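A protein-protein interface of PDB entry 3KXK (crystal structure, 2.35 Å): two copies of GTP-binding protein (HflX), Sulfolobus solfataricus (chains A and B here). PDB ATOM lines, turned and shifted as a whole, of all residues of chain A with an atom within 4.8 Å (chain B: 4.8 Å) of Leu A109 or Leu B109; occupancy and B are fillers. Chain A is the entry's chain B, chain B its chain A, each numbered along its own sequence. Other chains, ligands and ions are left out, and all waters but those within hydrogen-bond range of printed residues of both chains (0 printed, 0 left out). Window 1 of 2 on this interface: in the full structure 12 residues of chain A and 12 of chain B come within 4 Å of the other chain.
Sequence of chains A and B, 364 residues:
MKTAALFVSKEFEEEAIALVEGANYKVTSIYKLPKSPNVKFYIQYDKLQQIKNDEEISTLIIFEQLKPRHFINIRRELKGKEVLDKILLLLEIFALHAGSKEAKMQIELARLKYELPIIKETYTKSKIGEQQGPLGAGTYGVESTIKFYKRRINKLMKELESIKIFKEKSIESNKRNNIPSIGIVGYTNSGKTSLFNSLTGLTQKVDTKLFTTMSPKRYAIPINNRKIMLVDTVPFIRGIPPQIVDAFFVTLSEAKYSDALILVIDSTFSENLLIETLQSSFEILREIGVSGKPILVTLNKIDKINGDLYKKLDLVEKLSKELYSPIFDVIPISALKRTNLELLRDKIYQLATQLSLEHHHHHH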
ATOM      1  N   MET A 105     -18.412   1.856 -31.606  1.00  0.00           N
ATOM      2  CA  MET A 105     -18.163   2.489 -30.316  1.00  0.00           C
ATOM      3  C   MET A 105     -16.794   3.159 -30.267  1.00  0.00           C
ATOM      4  O   MET A 105     -16.679   4.317 -29.865  1.00  0.00           O
ATOM      5  CB  MET A 105     -18.291   1.462 -29.191  1.00  0.00           C
ATOM      6  CG  MET A 105     -19.650   0.786 -29.128  1.00  0.00           C
ATOM      7  SD  MET A 105     -19.737  -0.486 -27.853  1.00  0.00           S
ATOM      8  CE  MET A 105     -19.344   0.473 -26.394  1.00  0.00           C
ATOM      9  N   GLN A 106     -15.762   2.427 -30.673  1.00  0.00           N
ATOM     10  CA  GLN A 106     -14.405   2.962 -30.692  1.00  0.00           C
ATOM     11  C   GLN A 106     -14.325   4.240 -31.519  1.00  0.00           C
ATOM     12  O   GLN A 106     -13.682   5.212 -31.119  1.00  0.00           O
ATOM     13  CB  GLN A 106     -13.424   1.923 -31.238  1.00  0.00           C
ATOM     14  CG  GLN A 106     -13.085   0.808 -30.263  1.00  0.00           C
ATOM     15  CD  GLN A 106     -12.181   1.272 -29.136  1.00  0.00           C
ATOM     16  OE1 GLN A 106     -11.867   2.457 -29.023  1.00  0.00           O
ATOM     17  NE2 GLN A 106     -11.753   0.335 -28.298  1.00  0.00           N
ATOM     18  N   ILE A 107     -14.981   4.232 -32.674  1.00  0.00           N
ATOM     19  CA  ILE A 107     -15.001   5.395 -33.551  1.00  0.00           C
ATOM     20  C   ILE A 107     -15.705   6.570 -32.882  1.00  0.00           C
ATOM     21  O   ILE A 107     -15.206   7.695 -32.895  1.00  0.00           O
ATOM     22  CB  ILE A 107     -15.696   5.076 -34.885  1.00  0.00           C
ATOM     23  CG1 ILE A 107     -14.959   3.946 -35.607  1.00  0.00           C
ATOM     24  CG2 ILE A 107     -15.761   6.316 -35.761  1.00  0.00           C
ATOM     25  CD1 ILE A 107     -15.703   3.397 -36.801  1.00  0.00           C
ATOM     26  N   GLU A 108     -16.868   6.300 -32.296  1.00  0.00           N
ATOM     27  CA  GLU A 108     -17.639   7.333 -31.619  1.00  0.00           C
ATOM     28  C   GLU A 108     -16.895   7.863 -30.396  1.00  0.00           C
ATOM     29  O   GLU A 108     -16.943   9.056 -30.099  1.00  0.00           O
ATOM     30  CB  GLU A 108     -19.017   6.800 -31.216  1.00  0.00           C
ATOM     31  CG  GLU A 108     -19.915   7.831 -30.550  1.00  0.00           C
ATOM     32  CD  GLU A 108     -20.264   8.990 -31.465  1.00  0.00           C
ATOM     33  OE1 GLU A 108     -19.952   8.917 -32.673  1.00  0.00           O
ATOM     34  OE2 GLU A 108     -20.855   9.975 -30.976  1.00  0.00           O
ATOM     35  N   LEU A 109     -16.205   6.970 -29.693  1.00  0.00           N
ATOM     36  CA  LEU A 109     -15.398   7.356 -28.540  1.00  0.00           C
ATOM     37  C   LEU A 109     -14.349   8.390 -28.929  1.00  0.00           C
ATOM     38  O   LEU A 109     -14.204   9.419 -28.270  1.00  0.00           O
ATOM     39  CB  LEU A 109     -14.720   6.132 -27.921  1.00  0.00           C
ATOM     40  CG  LEU A 109     -15.563   5.284 -26.965  1.00  0.00           C
ATOM     41  CD1 LEU A 109     -14.873   3.963 -26.661  1.00  0.00           C
ATOM     42  CD2 LEU A 109     -15.841   6.054 -25.682  1.00  0.00           C
ATOM     43  N   ALA A 110     -13.621   8.109 -30.005  1.00  0.00           N
ATOM     44  CA  ALA A 110     -12.601   9.026 -30.497  1.00  0.00           C
ATOM     45  C   ALA A 110     -13.221  10.353 -30.921  1.00  0.00           C
ATOM     46  O   ALA A 110     -12.646  11.417 -30.693  1.00  0.00           O
ATOM     47  CB  ALA A 110     -11.839   8.401 -31.654  1.00  0.00           C
ATOM     48  N   ARG A 111     -14.395  10.283 -31.539  1.00  0.00           N
ATOM     49  CA  ARG A 111     -15.098  11.482 -31.980  1.00  0.00           C
ATOM     50  C   ARG A 111     -15.497  12.356 -30.797  1.00  0.00           C
ATOM     51  O   ARG A 111     -15.362  13.579 -30.842  1.00  0.00           O
ATOM     52  CB  ARG A 111     -16.336  11.114 -32.799  1.00  0.00           C
ATOM     53  CG  ARG A 111     -17.211  12.304 -33.149  1.00  0.00           C
ATOM     54  CD  ARG A 111     -18.504  11.871 -33.818  1.00  0.00           C
ATOM     55  NE  ARG A 111     -19.450  12.977 -33.921  1.00  0.00           N
ATOM     56  CZ  ARG A 111     -20.324  13.301 -32.973  1.00  0.00           C
ATOM     57  NH1 ARG A 111     -20.376  12.600 -31.848  1.00  0.00           N
ATOM     58  NH2 ARG A 111     -21.147  14.326 -33.148  1.00  0.00           N
ATOM     59  N   LEU A 112     -15.992  11.722 -29.738  1.00  0.00           N
ATOM     60  CA  LEU A 112     -16.402  12.439 -28.537  1.00  0.00           C
ATOM     61  C   LEU A 112     -15.200  13.037 -27.812  1.00  0.00           C
ATOM     62  O   LEU A 112     -15.218  14.204 -27.424  1.00  0.00           O
ATOM     63  CB  LEU A 112     -17.182  11.518 -27.597  1.00  0.00           C
ATOM     64  CG  LEU A 112     -18.527  11.001 -28.113  1.00  0.00           C
ATOM     65  CD1 LEU A 112     -19.134  10.018 -27.126  1.00  0.00           C
ATOM     66  CD2 LEU A 112     -19.481  12.155 -28.382  1.00  0.00           C
ATOM     67  N   LYS A 113     -14.158  12.231 -27.633  1.00  0.00           N
ATOM     68  CA  LYS A 113     -12.937  12.693 -26.980  1.00  0.00           C
ATOM     69  C   LYS A 113     -12.326  13.871 -27.729  1.00  0.00           C
ATOM     70  O   LYS A 113     -11.645  14.707 -27.138  1.00  0.00           O
ATOM     71  CB  LYS A 113     -11.911  11.562 -26.886  1.00  0.00           C
ATOM     72  CG  LYS A 113     -12.280  10.445 -25.927  1.00  0.00           C
ATOM     73  CD  LYS A 113     -11.175   9.401 -25.872  1.00  0.00           C
ATOM     74  CE  LYS A 113     -11.510   8.283 -24.899  1.00  0.00           C
ATOM     75  NZ  LYS A 113     -10.444   7.243 -24.872  1.00  0.00           N
ATOM     76  N   LEU A 116     -15.083  17.085 -27.295  1.00  0.00           N
ATOM     77  CA  LEU A 116     -15.206  17.682 -25.967  1.00  0.00           C
ATOM     78  C   LEU A 116     -14.345  18.934 -25.795  1.00  0.00           C
ATOM     79  O   LEU A 116     -14.844  19.974 -25.370  1.00  0.00           O
ATOM     80  CB  LEU A 116     -14.880  16.660 -24.875  1.00  0.00           C
ATOM     81  CG  LEU A 116     -15.905  15.551 -24.636  1.00  0.00           C
ATOM     82  CD1 LEU A 116     -15.350  14.506 -23.684  1.00  0.00           C
ATOM     83  CD2 LEU A 116     -17.206  16.130 -24.103  1.00  0.00           C
ATOM     84  N   LYS B 104     -24.278  15.919 -22.537  1.00  0.00           N
ATOM     85  CA  LYS B 104     -24.668  14.781 -23.362  1.00  0.00           C
ATOM     86  C   LYS B 104     -23.455  13.968 -23.793  1.00  0.00           C
ATOM     87  O   LYS B 104     -23.462  12.739 -23.719  1.00  0.00           O
ATOM     88  CB  LYS B 104     -25.426  15.256 -24.603  1.00  0.00           C
ATOM     89  CG  LYS B 104     -26.804  15.819 -24.324  1.00  0.00           C
ATOM     90  CD  LYS B 104     -27.472  16.322 -25.599  1.00  0.00           C
ATOM     91  CE  LYS B 104     -27.762  15.190 -26.582  1.00  0.00           C
ATOM     92  NZ  LYS B 104     -26.549  14.705 -27.300  1.00  0.00           N
ATOM     93  N   MET B 105     -22.419  14.662 -24.250  1.00  0.00           N
ATOM     94  CA  MET B 105     -21.210  14.007 -24.736  1.00  0.00           C
ATOM     95  C   MET B 105     -20.409  13.358 -23.610  1.00  0.00           C
ATOM     96  O   MET B 105     -19.872  12.264 -23.777  1.00  0.00           O
ATOM     97  CB  MET B 105     -20.339  14.995 -25.511  1.00  0.00           C
ATOM     98  CG  MET B 105     -20.909  15.391 -26.864  1.00  0.00           C
ATOM     99  SD  MET B 105     -19.899  16.635 -27.684  1.00  0.00           S
ATOM    100  CE  MET B 105     -18.273  15.921 -27.466  1.00  0.00           C
ATOM    101  N   GLN B 106     -20.327  14.039 -22.471  1.00  0.00           N
ATOM    102  CA  GLN B 106     -19.660  13.483 -21.298  1.00  0.00           C
ATOM    103  C   GLN B 106     -20.355  12.203 -20.850  1.00  0.00           C
ATOM    104  O   GLN B 106     -19.710  11.182 -20.616  1.00  0.00           O
ATOM    105  CB  GLN B 106     -19.650  14.497 -20.150  1.00  0.00           C
ATOM    106  CG  GLN B 106     -18.671  15.647 -20.328  1.00  0.00           C
ATOM    107  CD  GLN B 106     -17.224  15.219 -20.153  1.00  0.00           C
ATOM    108  OE1 GLN B 106     -16.941  14.073 -19.804  1.00  0.00           O
ATOM    109  NE2 GLN B 106     -16.301  16.143 -20.394  1.00  0.00           N
ATOM    110  N   ILE B 107     -21.678  12.270 -20.733  1.00  0.00           N
ATOM    111  CA  ILE B 107     -22.480  11.121 -20.333  1.00  0.00           C
ATOM    112  C   ILE B 107     -22.293   9.979 -21.322  1.00  0.00           C
ATOM    113  O   ILE B 107     -21.976   8.852 -20.939  1.00  0.00           O
ATOM    114  CB  ILE B 107     -23.973  11.489 -20.267  1.00  0.00           C
ATOM    115  CG1 ILE B 107     -24.192  12.627 -19.268  1.00  0.00           C
ATOM    116  CG2 ILE B 107     -24.809  10.274 -19.894  1.00  0.00           C
ATOM    117  CD1 ILE B 107     -25.570  13.250 -19.345  1.00  0.00           C
ATOM    118  N   GLU B 108     -22.488  10.291 -22.599  1.00  0.00           N
ATOM    119  CA  GLU B 108     -22.326   9.323 -23.677  1.00  0.00           C
ATOM    120  C   GLU B 108     -20.920   8.736 -23.701  1.00  0.00           C
ATOM    121  O   GLU B 108     -20.740   7.544 -23.945  1.00  0.00           O
ATOM    122  CB  GLU B 108     -22.633   9.983 -25.023  1.00  0.00           C
ATOM    123  CG  GLU B 108     -22.408   9.084 -26.229  1.00  0.00           C
ATOM    124  CD  GLU B 108     -23.346   7.892 -26.262  1.00  0.00           C
ATOM    125  OE1 GLU B 108     -24.135   7.718 -25.308  1.00  0.00           O
ATOM    126  OE2 GLU B 108     -23.293   7.129 -27.247  1.00  0.00           O
ATOM    127  N   LEU B 109     -19.926   9.585 -23.462  1.00  0.00           N
ATOM    128  CA  LEU B 109     -18.541   9.139 -23.411  1.00  0.00           C
ATOM    129  C   LEU B 109     -18.363   8.106 -22.307  1.00  0.00           C
ATOM    130  O   LEU B 109     -17.854   7.010 -22.542  1.00  0.00           O
ATOM    131  CB  LEU B 109     -17.601  10.319 -23.163  1.00  0.00           C
ATOM    132  CG  LEU B 109     -16.127   9.940 -23.014  1.00  0.00           C
ATOM    133  CD1 LEU B 109     -15.594   9.378 -24.321  1.00  0.00           C
ATOM    134  CD2 LEU B 109     -15.305  11.137 -22.566  1.00  0.00           C
ATOM    135  N   ALA B 110     -18.789   8.467 -21.101  1.00  0.00           N
ATOM    136  CA  ALA B 110     -18.690   7.576 -19.953  1.00  0.00           C
ATOM    137  C   ALA B 110     -19.440   6.274 -20.208  1.00  0.00           C
ATOM    138  O   ALA B 110     -18.957   5.195 -19.864  1.00  0.00           O
ATOM    139  CB  ALA B 110     -19.222   8.259 -18.704  1.00  0.00           C
ATOM    140  N   ARG B 111     -20.618   6.378 -20.816  1.00  0.00           N
ATOM    141  CA  ARG B 111     -21.412   5.196 -21.132  1.00  0.00           C
ATOM    142  C   ARG B 111     -20.680   4.307 -22.128  1.00  0.00           C
ATOM    143  O   ARG B 111     -20.487   3.115 -21.884  1.00  0.00           O
ATOM    144  CB  ARG B 111     -22.783   5.582 -21.690  1.00  0.00           C
ATOM    145  CG  ARG B 111     -23.677   4.384 -21.972  1.00  0.00           C
ATOM    146  CD  ARG B 111     -25.035   4.804 -22.535  1.00  0.00           C
ATOM    147  NE  ARG B 111     -24.929   5.334 -23.892  1.00  0.00           N
ATOM    148  CZ  ARG B 111     -24.836   4.579 -24.982  1.00  0.00           C
ATOM    149  NH1 ARG B 111     -24.833   3.256 -24.875  1.00  0.00           N
ATOM    150  NH2 ARG B 111     -24.740   5.149 -26.176  1.00  0.00           N
ATOM    151  N   LEU B 112     -20.283   4.894 -23.254  1.00  0.00           N
ATOM    152  CA  LEU B 112     -19.519   4.174 -24.264  1.00  0.00           C
ATOM    153  C   LEU B 112     -18.256   3.609 -23.647  1.00  0.00           C
ATOM    154  O   LEU B 112     -17.798   2.527 -24.017  1.00  0.00           O
ATOM    155  CB  LEU B 112     -19.158   5.089 -25.427  1.00  0.00           C
ATOM    156  CG  LEU B 112     -20.321   5.508 -26.317  1.00  0.00           C
ATOM    157  CD1 LEU B 112     -19.826   6.443 -27.404  1.00  0.00           C
ATOM    158  CD2 LEU B 112     -20.992   4.287 -26.917  1.00  0.00           C
ATOM    159  N   LYS B 113     -17.692   4.345 -22.699  1.00  0.00           N
ATOM    160  CA  LYS B 113     -16.540   3.848 -21.974  1.00  0.00           C
ATOM    161  C   LYS B 113     -16.905   2.593 -21.193  1.00  0.00           C
ATOM    162  O   LYS B 113     -16.283   1.548 -21.367  1.00  0.00           O
ATOM    163  CB  LYS B 113     -15.975   4.921 -21.047  1.00  0.00           C
ATOM    164  CG  LYS B 113     -15.006   5.860 -21.737  1.00  0.00           C
ATOM    165  CD  LYS B 113     -14.333   6.755 -20.726  1.00  0.00           C
ATOM    166  CE  LYS B 113     -13.400   7.736 -21.395  1.00  0.00           C
ATOM    167  NZ  LYS B 113     -12.740   8.578 -20.370  1.00  0.00           N
ATOM    168  N   LEU B 116     -17.726  -0.171 -23.323  1.00  0.00           N
ATOM    169  CA  LEU B 116     -16.589  -0.587 -24.137  1.00  0.00           C
ATOM    170  C   LEU B 116     -15.938  -1.869 -23.589  1.00  0.00           C
ATOM    171  O   LEU B 116     -15.925  -2.883 -24.282  1.00  0.00           O
ATOM    172  CB  LEU B 116     -15.581   0.556 -24.311  1.00  0.00           C
ATOM    173  CG  LEU B 116     -14.464   0.373 -25.342  1.00  0.00           C
ATOM    174  CD1 LEU B 116     -13.288  -0.385 -24.748  1.00  0.00           C
ATOM    175  CD2 LEU B 116     -14.988  -0.324 -26.591  1.00  0.00           C
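The side-chain carboxylate of Glu B108 is in salt-bridge range of the guanidinium group of Arg B111, at 2.7 Å.
NH1 of Arg A111 lies within salt-bridge range of OE2 of Glu A108 (2.8 Å).
Among the printed residues, pairs that only touch across the chains: Met A105 with Leu B112, Met A105 with Leu B116, Gln A106 with Leu B116, Glu A108 with Leu B112, Leu A109 with Leu B109, Leu A109 with Leu B112, Leu A109 with Lys B113, Leu A109 with Leu B116, Leu A112 with Met B105, Leu A112 with Glu B108, Leu A112 with Leu B109, Leu A112 with Leu B112, Lys A113 with Leu B109, Leu A116 with Met B105, Leu A116 with Gln B106 and Leu A116 with Leu B109.
Leu A109 touches four residues of chain B.
Printed residues of chain B within 4 Å of Leu A116: Met B105 (3.4 Å), Gln B106 (3.8 Å) and Leu B109 (3.5 Å).
Lys B104 touches none of the printed residues of chain A.
Of chain A, only Leu A109, Leu A112, Lys A113 and Leu A116 come within 4 Å of Leu B109.
Ala B110 touches none of the printed residues of chain A.
Of the printed residues of chain A, Lys B113 touches Leu A109 (3.9 Å).
The nearest printed residue of chain B that does not touch Gln A106 is Leu B112 (6.6 Å).
Hydrophobic or aromatic side chains of chain B that line the printed part of chain A: Met B105, Leu B109, Leu B112 and Leu B116.
Of the 10 printed residues of chain A, 7 touch a printed residue of chain B.
Hydrophobic or aromatic side chains of chain A within 4 Å of the printed part of chain B: Met A105, Leu A109, Leu A112 and Leu A116.
Among the printed residues, 16 pairs touch across the chains.
Among the printed residues, no Asp or Glu carboxylate lies within 4 Å of a Lys or Arg side-chain nitrogen of the other chain.
Met A105 touches Leu B116, and with the chains exchanged Leu A116 touches Met B105.
Leu A109 touches its own counterpart, Leu B109.
Leu A109 touches Leu B112, and with the chains exchanged Leu A112 touches Leu B109.
Leu A109 touches Lys B113, and with the chains exchanged Lys A113 touches Leu B109.
Positions printed for both chains: 105, 106, 107, 108, 109, 110, 111, 112, 113 and 116.
Of the 16 pairs that touch across the chains among the printed residues, 16 have their exchanged pair printed and touching as well.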
